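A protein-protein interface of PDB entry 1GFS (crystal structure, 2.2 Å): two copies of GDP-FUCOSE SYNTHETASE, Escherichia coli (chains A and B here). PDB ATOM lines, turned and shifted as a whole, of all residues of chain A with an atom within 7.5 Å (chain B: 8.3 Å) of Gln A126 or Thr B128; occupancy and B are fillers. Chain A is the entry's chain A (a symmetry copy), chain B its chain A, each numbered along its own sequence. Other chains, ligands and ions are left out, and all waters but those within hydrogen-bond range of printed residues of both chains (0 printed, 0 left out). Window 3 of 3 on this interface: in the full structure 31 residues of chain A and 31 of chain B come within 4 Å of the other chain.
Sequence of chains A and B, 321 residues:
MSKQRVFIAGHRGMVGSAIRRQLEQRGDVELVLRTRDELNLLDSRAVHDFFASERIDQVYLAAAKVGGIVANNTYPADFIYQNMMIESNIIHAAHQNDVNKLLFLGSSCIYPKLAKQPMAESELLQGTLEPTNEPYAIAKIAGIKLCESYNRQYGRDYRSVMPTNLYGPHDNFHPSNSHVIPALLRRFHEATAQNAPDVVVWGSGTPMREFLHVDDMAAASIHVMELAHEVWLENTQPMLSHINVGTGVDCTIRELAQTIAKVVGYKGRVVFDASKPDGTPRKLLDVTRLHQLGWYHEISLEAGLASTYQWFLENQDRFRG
Printed residues of chain B within 4 Å of Leu A125: Leu B125, Gly B127 and Thr B128.
Of chain B, only Gln B126 (3.8 Å) and Thr B128 (3.1 Å) come within 4 Å of Gln A126.
Gly A127 touches just one residue of chain B: Leu B125 (3.2 Å).
Of the printed residues of chain B, Thr A128 touches Leu B125 (3.7 Å) and Gln B126 (3.1 Å).
Of the printed residues of chain A, Leu B125 touches Leu A125, Gly A127 and Thr A128.
Of the printed residues of chain A, Gln B126 touches Gln A126 and Thr A128.
Of the printed residues of chain A, Gly B127 touches Leu A125.
Thr B128 touches just these residues of chain A: Leu A125 (3.7 Å) and Gln A126 (3.1 Å).
Glu B134 touches none of the printed residues of chain A.
The nearest residue of chain B that does not touch Gln A126 is Gly B127 (4.3 Å).
The nearest residue of chain A that does not touch Thr B128 is Leu A124 (4.6 Å).
The nearest printed residue of chain B that does not touch Leu A125 is Leu B129 (4.5 Å).
Of the 17 printed residues of chain A, 4 touch a printed residue of chain B.
Among the printed residues, 8 pairs touch across the chains.
Leu A125 touches its own counterpart, Leu B125.
Leu A125 touches Gly B127, and with the chains exchanged Gly A127 touches Leu B125.
Gln B126 touches its own counterpart, Gln A126.
Gln A126 touches Thr B128, and with the chains exchanged Thr A128 touches Gln B126.
Positions printed for both chains: 110, 111, 112, 113, 114, 115, 123, 125, 126, 127, 128 and 129.
Of the 8 pairs that touch across the chains among the printed residues, 8 have their exchanged pair printed and touching as well.
Leu B125 touches Leu A125 (CD2 to CD2, 3.97 Å).
Thr B128 touches Leu A125.
Gln A126 touches Gln B126 (O to O, 3.8 Å).
Gln A126 touches Thr B128.
O of Leu B125 touches N of Thr A128, 3.7 Å away.
Gln B126 touches Thr A128.
NE2 of Gln A126 sits at hydrogen-bond distance from O of Ser A122 (3.3 Å).
The backbone NH (N) of Lys B113 lies within hydrogen-bond range of the backbone carbonyl oxygen (O) of Thr B128 (2.8 Å).
The backbone carbonyl oxygen (O) of Thr A128 sits at hydrogen-bond distance from the backbone NH (N) of Lys A113 (2.8 Å).
The backbone carbonyl oxygen of Leu B125 lies close to the backbone carbonyl oxygen of Gly A127, 3.2 Å away.
O of Leu A125 sits close to O of Gly B127 (3.2 Å).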
ATOM      1  N   ILE A 110      12.040  18.984  29.827  1.00  0.00           N
ATOM      2  CA  ILE A 110      12.163  18.966  28.373  1.00  0.00           C
ATOM      3  C   ILE A 110      12.708  17.655  27.803  1.00  0.00           C
ATOM      4  O   ILE A 110      12.634  17.428  26.600  1.00  0.00           O
ATOM      5  CB  ILE A 110      13.090  20.113  27.865  1.00  0.00           C
ATOM      6  CG1 ILE A 110      14.548  19.831  28.273  1.00  0.00           C
ATOM      7  CG2 ILE A 110      12.632  21.458  28.415  1.00  0.00           C
ATOM      8  CD1 ILE A 110      15.611  20.581  27.468  1.00  0.00           C
ATOM      9  N   TYR A 111      13.298  16.811  28.638  1.00  0.00           N
ATOM     10  CA  TYR A 111      13.862  15.570  28.130  1.00  0.00           C
ATOM     11  C   TYR A 111      12.853  14.452  27.973  1.00  0.00           C
ATOM     12  O   TYR A 111      11.841  14.423  28.669  1.00  0.00           O
ATOM     13  CB  TYR A 111      15.043  15.130  28.987  1.00  0.00           C
ATOM     14  CG  TYR A 111      16.234  16.006  28.756  1.00  0.00           C
ATOM     15  CD1 TYR A 111      16.868  16.042  27.503  1.00  0.00           C
ATOM     16  CD2 TYR A 111      16.715  16.828  29.760  1.00  0.00           C
ATOM     17  CE1 TYR A 111      17.958  16.884  27.264  1.00  0.00           C
ATOM     18  CE2 TYR A 111      17.808  17.675  29.539  1.00  0.00           C
ATOM     19  CZ  TYR A 111      18.425  17.697  28.294  1.00  0.00           C
ATOM     20  OH  TYR A 111      19.527  18.505  28.115  1.00  0.00           O
ATOM     21  N   PRO A 112      13.101  13.536  27.020  1.00  0.00           N
ATOM     22  CA  PRO A 112      12.206  12.402  26.770  1.00  0.00           C
ATOM     23  C   PRO A 112      11.983  11.635  28.069  1.00  0.00           C
ATOM     24  O   PRO A 112      12.871  11.577  28.913  1.00  0.00           O
ATOM     25  CB  PRO A 112      12.997  11.568  25.775  1.00  0.00           C
ATOM     26  CG  PRO A 112      13.781  12.597  25.021  1.00  0.00           C
ATOM     27  CD  PRO A 112      14.259  13.500  26.111  1.00  0.00           C
ATOM     28  N   LYS A 113      10.785  11.088  28.241  1.00  0.00           N
ATOM     29  CA  LYS A 113      10.445  10.325  29.438  1.00  0.00           C
ATOM     30  C   LYS A 113      11.407   9.134  29.634  1.00  0.00           C
ATOM     31  O   LYS A 113      11.906   8.885  30.742  1.00  0.00           O
ATOM     32  CB  LYS A 113       9.000   9.829  29.327  1.00  0.00           C
ATOM     33  CG  LYS A 113       8.516   9.076  30.539  1.00  0.00           C
ATOM     34  CD  LYS A 113       7.233   8.314  30.244  1.00  0.00           C
ATOM     35  CE  LYS A 113       6.838   7.460  31.455  1.00  0.00           C
ATOM     36  NZ  LYS A 113       5.660   6.590  31.177  1.00  0.00           N
ATOM     37  N   LEU A 114      11.697   8.440  28.536  1.00  0.00           N
ATOM     38  CA  LEU A 114      12.581   7.276  28.551  1.00  0.00           C
ATOM     39  C   LEU A 114      13.983   7.553  28.013  1.00  0.00           C
ATOM     40  O   LEU A 114      14.562   6.722  27.323  1.00  0.00           O
ATOM     41  CB  LEU A 114      11.937   6.133  27.764  1.00  0.00           C
ATOM     42  CG  LEU A 114      10.580   5.701  28.322  1.00  0.00           C
ATOM     43  CD1 LEU A 114       9.962   4.680  27.396  1.00  0.00           C
ATOM     44  CD2 LEU A 114      10.723   5.150  29.746  1.00  0.00           C
ATOM     45  N   ALA A 115      14.539   8.704  28.358  1.00  0.00           N
ATOM     46  CA  ALA A 115      15.871   9.073  27.912  1.00  0.00           C
ATOM     47  C   ALA A 115      16.970   8.171  28.505  1.00  0.00           C
ATOM     48  O   ALA A 115      16.762   7.492  29.510  1.00  0.00           O
ATOM     49  CB  ALA A 115      16.139  10.529  28.261  1.00  0.00           C
ATOM     50  N   LYS A 116      18.124   8.150  27.845  1.00  0.00           N
ATOM     51  CA  LYS A 116      19.283   7.375  28.275  1.00  0.00           C
ATOM     52  C   LYS A 116      19.856   8.141  29.464  1.00  0.00           C
ATOM     53  O   LYS A 116      19.928   9.368  29.417  1.00  0.00           O
ATOM     54  CB  LYS A 116      20.307   7.327  27.132  1.00  0.00           C
ATOM     55  CG  LYS A 116      21.591   6.557  27.426  1.00  0.00           C
ATOM     56  CD  LYS A 116      22.688   6.948  26.427  1.00  0.00           C
ATOM     57  CE  LYS A 116      24.014   6.229  26.696  1.00  0.00           C
ATOM     58  NZ  LYS A 116      23.994   4.784  26.286  1.00  0.00           N
ATOM     59  N   ALA A 120      22.405  13.522  28.430  1.00  0.00           N
ATOM     60  CA  ALA A 120      23.258  14.524  27.816  1.00  0.00           C
ATOM     61  C   ALA A 120      22.330  15.464  27.044  1.00  0.00           C
ATOM     62  O   ALA A 120      21.169  15.130  26.787  1.00  0.00           O
ATOM     63  CB  ALA A 120      24.263  13.865  26.878  1.00  0.00           C
ATOM     64  N   GLU A 121      22.843  16.643  26.703  1.00  0.00           N
ATOM     65  CA  GLU A 121      22.083  17.655  25.979  1.00  0.00           C
ATOM     66  C   GLU A 121      21.471  17.158  24.679  1.00  0.00           C
ATOM     67  O   GLU A 121      20.370  17.584  24.285  1.00  0.00           O
ATOM     68  CB  GLU A 121      22.966  18.868  25.713  1.00  0.00           C
ATOM     69  CG  GLU A 121      23.228  19.723  26.950  1.00  0.00           C
ATOM     70  CD  GLU A 121      24.412  19.267  27.809  1.00  0.00           C
ATOM     71  OE1 GLU A 121      24.972  18.169  27.593  1.00  0.00           O
ATOM     72  OE2 GLU A 121      24.794  20.032  28.717  1.00  0.00           O
ATOM     73  N   SER A 122      22.164  16.219  24.046  1.00  0.00           N
ATOM     74  CA  SER A 122      21.743  15.628  22.774  1.00  0.00           C
ATOM     75  C   SER A 122      20.539  14.700  22.895  1.00  0.00           C
ATOM     76  O   SER A 122      20.081  14.120  21.910  1.00  0.00           O
ATOM     77  CB  SER A 122      22.910  14.860  22.153  1.00  0.00           C
ATOM     78  OG  SER A 122      23.385  13.876  23.056  1.00  0.00           O
ATOM     79  N   GLU A 123      20.025  14.566  24.106  1.00  0.00           N
ATOM     80  CA  GLU A 123      18.879  13.721  24.359  1.00  0.00           C
ATOM     81  C   GLU A 123      17.595  14.507  24.047  1.00  0.00           C
ATOM     82  O   GLU A 123      16.493  13.943  23.968  1.00  0.00           O
ATOM     83  CB  GLU A 123      18.919  13.295  25.817  1.00  0.00           C
ATOM     84  CG  GLU A 123      18.347  11.939  26.069  1.00  0.00           C
ATOM     85  CD  GLU A 123      19.092  10.836  25.350  1.00  0.00           C
ATOM     86  OE1 GLU A 123      20.335  10.817  25.406  1.00  0.00           O
ATOM     87  OE2 GLU A 123      18.423   9.976  24.744  1.00  0.00           O
ATOM     88  N   LEU A 124      17.757  15.811  23.840  1.00  0.00           N
ATOM     89  CA  LEU A 124      16.640  16.685  23.531  1.00  0.00           C
ATOM     90  C   LEU A 124      15.928  16.244  22.262  1.00  0.00           C
ATOM     91  O   LEU A 124      16.575  15.960  21.261  1.00  0.00           O
ATOM     92  CB  LEU A 124      17.126  18.119  23.351  1.00  0.00           C
ATOM     93  CG  LEU A 124      15.984  19.119  23.201  1.00  0.00           C
ATOM     94  CD1 LEU A 124      15.240  19.184  24.517  1.00  0.00           C
ATOM     95  CD2 LEU A 124      16.507  20.480  22.830  1.00  0.00           C
ATOM     96  N   LEU A 125      14.599  16.169  22.326  1.00  0.00           N
ATOM     97  CA  LEU A 125      13.759  15.785  21.194  1.00  0.00           C
ATOM     98  C   LEU A 125      13.949  14.352  20.672  1.00  0.00           C
ATOM     99  O   LEU A 125      13.491  14.028  19.575  1.00  0.00           O
ATOM    100  CB  LEU A 125      13.915  16.804  20.047  1.00  0.00           C
ATOM    101  CG  LEU A 125      13.323  18.204  20.257  1.00  0.00           C
ATOM    102  CD1 LEU A 125      13.810  19.166  19.194  1.00  0.00           C
ATOM    103  CD2 LEU A 125      11.812  18.141  20.220  1.00  0.00           C
ATOM    104  N   GLN A 126      14.555  13.485  21.481  1.00  0.00           N
ATOM    105  CA  GLN A 126      14.811  12.092  21.091  1.00  0.00           C
ATOM    106  C   GLN A 126      13.707  11.084  21.405  1.00  0.00           C
ATOM    107  O   GLN A 126      13.866   9.888  21.163  1.00  0.00           O
ATOM    108  CB  GLN A 126      16.089  11.597  21.759  1.00  0.00           C
ATOM    109  CG  GLN A 126      17.323  12.310  21.318  1.00  0.00           C
ATOM    110  CD  GLN A 126      17.760  11.880  19.952  1.00  0.00           C
ATOM    111  OE1 GLN A 126      16.936  11.590  19.080  1.00  0.00           O
ATOM    112  NE2 GLN A 126      19.071  11.813  19.750  1.00  0.00           N
ATOM    113  N   GLY A 127      12.599  11.542  21.961  1.00  0.00           N
ATOM    114  CA  GLY A 127      11.543  10.616  22.295  1.00  0.00           C
ATOM    115  C   GLY A 127      10.389  11.360  22.911  1.00  0.00           C
ATOM    116  O   GLY A 127      10.469  12.560  23.167  1.00  0.00           O
ATOM    117  N   THR A 128       9.325  10.631  23.201  1.00  0.00           N
ATOM    118  CA  THR A 128       8.137  11.249  23.750  1.00  0.00           C
ATOM    119  C   THR A 128       8.308  11.799  25.165  1.00  0.00           C
ATOM    120  O   THR A 128       9.059  11.257  25.986  1.00  0.00           O
ATOM    121  CB  THR A 128       6.887  10.307  23.639  1.00  0.00           C
ATOM    122  OG1 THR A 128       6.973   9.264  24.609  1.00  0.00           O
ATOM    123  CG2 THR A 128       6.805   9.681  22.244  1.00  0.00           C
ATOM    124  N   LEU A 129       7.616  12.908  25.409  1.00  0.00           N
ATOM    125  CA  LEU A 129       7.631  13.599  26.684  1.00  0.00           C
ATOM    126  C   LEU A 129       6.671  12.990  27.712  1.00  0.00           C
ATOM    127  O   LEU A 129       5.740  12.262  27.360  1.00  0.00           O
ATOM    128  CB  LEU A 129       7.255  15.070  26.460  1.00  0.00           C
ATOM    129  CG  LEU A 129       8.173  15.867  25.531  1.00  0.00           C
ATOM    130  CD1 LEU A 129       7.527  17.180  25.098  1.00  0.00           C
ATOM    131  CD2 LEU A 129       9.493  16.109  26.238  1.00  0.00           C
ATOM    132  N   CYS B 109       6.602  18.534   7.842  1.00  0.00           N
ATOM    133  CA  CYS B 109       7.943  18.764   8.387  1.00  0.00           C
ATOM    134  C   CYS B 109       8.065  18.450   9.861  1.00  0.00           C
ATOM    135  O   CYS B 109       9.171  18.324  10.375  1.00  0.00           O
ATOM    136  CB  CYS B 109       8.328  20.228   8.204  1.00  0.00           C
ATOM    137  SG  CYS B 109       8.006  20.841   6.569  1.00  0.00           S
ATOM    138  N   ILE B 110       6.936  18.384  10.550  1.00  0.00           N
ATOM    139  CA  ILE B 110       6.922  18.115  11.984  1.00  0.00           C
ATOM    140  C   ILE B 110       7.404  16.714  12.367  1.00  0.00           C
ATOM    141  O   ILE B 110       7.663  16.450  13.535  1.00  0.00           O
ATOM    142  CB  ILE B 110       5.493  18.295  12.584  1.00  0.00           C
ATOM    143  CG1 ILE B 110       4.566  17.173  12.079  1.00  0.00           C
ATOM    144  CG2 ILE B 110       4.926  19.661  12.221  1.00  0.00           C
ATOM    145  CD1 ILE B 110       3.311  16.933  12.919  1.00  0.00           C
ATOM    146  N   TYR B 111       7.478  15.799  11.411  1.00  0.00           N
ATOM    147  CA  TYR B 111       7.897  14.445  11.738  1.00  0.00           C
ATOM    148  C   TYR B 111       9.397  14.261  11.806  1.00  0.00           C
ATOM    149  O   TYR B 111      10.145  14.991  11.159  1.00  0.00           O
ATOM    150  CB  TYR B 111       7.260  13.444  10.782  1.00  0.00           C
ATOM    151  CG  TYR B 111       5.799  13.280  11.063  1.00  0.00           C
ATOM    152  CD1 TYR B 111       5.357  12.739  12.281  1.00  0.00           C
ATOM    153  CD2 TYR B 111       4.851  13.695  10.144  1.00  0.00           C
ATOM    154  CE1 TYR B 111       3.995  12.617  12.570  1.00  0.00           C
ATOM    155  CE2 TYR B 111       3.483  13.577  10.416  1.00  0.00           C
ATOM    156  CZ  TYR B 111       3.061  13.037  11.625  1.00  0.00           C
ATOM    157  OH  TYR B 111       1.710  12.889  11.849  1.00  0.00           O
ATOM    158  N   PRO B 112       9.859  13.303  12.629  1.00  0.00           N
ATOM    159  CA  PRO B 112      11.289  13.021  12.782  1.00  0.00           C
ATOM    160  C   PRO B 112      11.903  12.754  11.412  1.00  0.00           C
ATOM    161  O   PRO B 112      11.236  12.229  10.527  1.00  0.00           O
ATOM    162  CB  PRO B 112      11.290  11.760  13.633  1.00  0.00           C
ATOM    163  CG  PRO B 112      10.058  11.918  14.468  1.00  0.00           C
ATOM    164  CD  PRO B 112       9.054  12.404  13.475  1.00  0.00           C
ATOM    165  N   LYS B 113      13.155  13.159  11.230  1.00  0.00           N
ATOM    166  CA  LYS B 113      13.859  12.961   9.966  1.00  0.00           C
ATOM    167  C   LYS B 113      13.912  11.466   9.585  1.00  0.00           C
ATOM    168  O   LYS B 113      13.651  11.087   8.434  1.00  0.00           O
ATOM    169  CB  LYS B 113      15.275  13.531  10.083  1.00  0.00           C
ATOM    170  CG  LYS B 113      16.080  13.437   8.812  1.00  0.00           C
ATOM    171  CD  LYS B 113      17.559  13.681   9.071  1.00  0.00           C
ATOM    172  CE  LYS B 113      18.362  13.454   7.786  1.00  0.00           C
ATOM    173  NZ  LYS B 113      19.834  13.551   8.010  1.00  0.00           N
ATOM    174  N   LEU B 114      14.202  10.627  10.578  1.00  0.00           N
ATOM    175  CA  LEU B 114      14.305   9.183  10.383  1.00  0.00           C
ATOM    176  C   LEU B 114      13.095   8.399  10.885  1.00  0.00           C
ATOM    177  O   LEU B 114      13.240   7.318  11.443  1.00  0.00           O
ATOM    178  CB  LEU B 114      15.578   8.663  11.055  1.00  0.00           C
ATOM    179  CG  LEU B 114      16.856   9.305  10.510  1.00  0.00           C
ATOM    180  CD1 LEU B 114      18.035   8.843  11.334  1.00  0.00           C
ATOM    181  CD2 LEU B 114      17.047   8.973   9.027  1.00  0.00           C
ATOM    182  N   ALA B 115      11.903   8.929  10.656  1.00  0.00           N
ATOM    183  CA  ALA B 115      10.679   8.271  11.083  1.00  0.00           C
ATOM    184  C   ALA B 115      10.423   6.950  10.336  1.00  0.00           C
ATOM    185  O   ALA B 115      10.980   6.703   9.267  1.00  0.00           O
ATOM    186  CB  ALA B 115       9.504   9.218  10.899  1.00  0.00           C
ATOM    187  N   GLU B 123       4.115   9.153  15.328  1.00  0.00           N
ATOM    188  CA  GLU B 123       5.520   9.313  15.028  1.00  0.00           C
ATOM    189  C   GLU B 123       5.981  10.704  15.490  1.00  0.00           C
ATOM    190  O   GLU B 123       7.183  11.002  15.551  1.00  0.00           O
ATOM    191  CB  GLU B 123       5.704   9.145  13.529  1.00  0.00           C
ATOM    192  CG  GLU B 123       7.016   8.545  13.142  1.00  0.00           C
ATOM    193  CD  GLU B 123       7.217   7.150  13.689  1.00  0.00           C
ATOM    194  OE1 GLU B 123       6.293   6.323  13.574  1.00  0.00           O
ATOM    195  OE2 GLU B 123       8.314   6.879  14.216  1.00  0.00           O
ATOM    196  N   LEU B 125       7.212  13.706  17.533  1.00  0.00           N
ATOM    197  CA  LEU B 125       8.148  13.838  18.647  1.00  0.00           C
ATOM    198  C   LEU B 125       8.972  12.586  18.985  1.00  0.00           C
ATOM    199  O   LEU B 125       9.580  12.515  20.054  1.00  0.00           O
ATOM    200  CB  LEU B 125       7.411  14.354  19.901  1.00  0.00           C
ATOM    201  CG  LEU B 125       6.923  15.809  19.889  1.00  0.00           C
ATOM    202  CD1 LEU B 125       5.972  16.073  21.035  1.00  0.00           C
ATOM    203  CD2 LEU B 125       8.101  16.752  19.986  1.00  0.00           C
ATOM    204  N   GLN B 126       9.052  11.641  18.051  1.00  0.00           N
ATOM    205  CA  GLN B 126       9.797  10.391  18.257  1.00  0.00           C
ATOM    206  C   GLN B 126      11.276  10.408  17.875  1.00  0.00           C
ATOM    207  O   GLN B 126      11.955   9.386  17.965  1.00  0.00           O
ATOM    208  CB  GLN B 126       9.133   9.262  17.478  1.00  0.00           C
ATOM    209  CG  GLN B 126       7.757   8.924  17.945  1.00  0.00           C
ATOM    210  CD  GLN B 126       7.774   8.152  19.229  1.00  0.00           C
ATOM    211  OE1 GLN B 126       8.624   8.376  20.094  1.00  0.00           O
ATOM    212  NE2 GLN B 126       6.844   7.215  19.360  1.00  0.00           N
ATOM    213  N   GLY B 127      11.781  11.545  17.429  1.00  0.00           N
ATOM    214  CA  GLY B 127      13.167  11.594  17.036  1.00  0.00           C
ATOM    215  C   GLY B 127      13.515  12.981  16.566  1.00  0.00           C
ATOM    216  O   GLY B 127      12.653  13.850  16.453  1.00  0.00           O
ATOM    217  N   THR B 128      14.782  13.175  16.239  1.00  0.00           N
ATOM    218  CA  THR B 128      15.241  14.484  15.823  1.00  0.00           C
ATOM    219  C   THR B 128      14.686  14.950  14.478  1.00  0.00           C
ATOM    220  O   THR B 128      14.442  14.151  13.565  1.00  0.00           O
ATOM    221  CB  THR B 128      16.805  14.596  15.877  1.00  0.00           C
ATOM    222  OG1 THR B 128      17.384  13.880  14.786  1.00  0.00           O
ATOM    223  CG2 THR B 128      17.343  14.016  17.189  1.00  0.00           C
ATOM    224  N   LEU B 129      14.463  16.258  14.402  1.00  0.00           N
ATOM    225  CA  LEU B 129      13.938  16.915  13.220  1.00  0.00           C
ATOM    226  C   LEU B 129      15.014  17.218  12.170  1.00  0.00           C
ATOM    227  O   LEU B 129      16.208  17.249  12.475  1.00  0.00           O
ATOM    228  CB  LEU B 129      13.261  18.228  13.636  1.00  0.00           C
ATOM    229  CG  LEU B 129      12.090  18.103  14.611  1.00  0.00           C
ATOM    230  CD1 LEU B 129      11.729  19.450  15.227  1.00  0.00           C
ATOM    231  CD2 LEU B 129      10.907  17.498  13.879  1.00  0.00           C
ATOM    232  N   GLU B 130      14.558  17.416  10.933  1.00  0.00           N
ATOM    233  CA  GLU B 130      15.398  17.788   9.807  1.00  0.00           C
ATOM    234  C   GLU B 130      15.885  19.206  10.161  1.00  0.00           C
ATOM    235  O   GLU B 130      15.080  20.107  10.408  1.00  0.00           O
ATOM    236  CB  GLU B 130      14.536  17.774   8.530  1.00  0.00           C
ATOM    237  CG  GLU B 130      15.155  18.402   7.276  1.00  0.00           C
ATOM    238  CD  GLU B 130      16.544  17.862   6.947  1.00  0.00           C
ATOM    239  OE1 GLU B 130      16.672  16.619   6.783  1.00  0.00           O
ATOM    240  OE2 GLU B 130      17.496  18.691   6.857  1.00  0.00           O
ATOM    241  N   PRO B 131      17.213  19.405  10.249  1.00  0.00           N
ATOM    242  CA  PRO B 131      17.786  20.714  10.593  1.00  0.00           C
ATOM    243  C   PRO B 131      17.201  21.901   9.830  1.00  0.00           C
ATOM    244  O   PRO B 131      16.880  22.932  10.427  1.00  0.00           O
ATOM    245  CB  PRO B 131      19.272  20.522  10.291  1.00  0.00           C
ATOM    246  CG  PRO B 131      19.492  19.078  10.625  1.00  0.00           C
ATOM    247  CD  PRO B 131      18.281  18.422   9.980  1.00  0.00           C
ATOM    248  N   GLU B 134      13.810  22.654  11.307  1.00  0.00           N
ATOM    249  CA  GLU B 134      13.672  22.694  12.744  1.00  0.00           C
ATOM    250  C   GLU B 134      12.888  23.866  13.360  1.00  0.00           C
ATOM    251  O   GLU B 134      11.932  23.632  14.088  1.00  0.00           O
ATOM    252  CB  GLU B 134      15.019  22.499  13.426  1.00  0.00           C
ATOM    253  CG  GLU B 134      14.876  22.458  14.925  1.00  0.00           C
ATOM    254  CD  GLU B 134      16.116  21.992  15.622  1.00  0.00           C
ATOM    255  OE1 GLU B 134      16.334  20.764  15.664  1.00  0.00           O
ATOM    256  OE2 GLU B 134      16.862  22.850  16.137  1.00  0.00           O
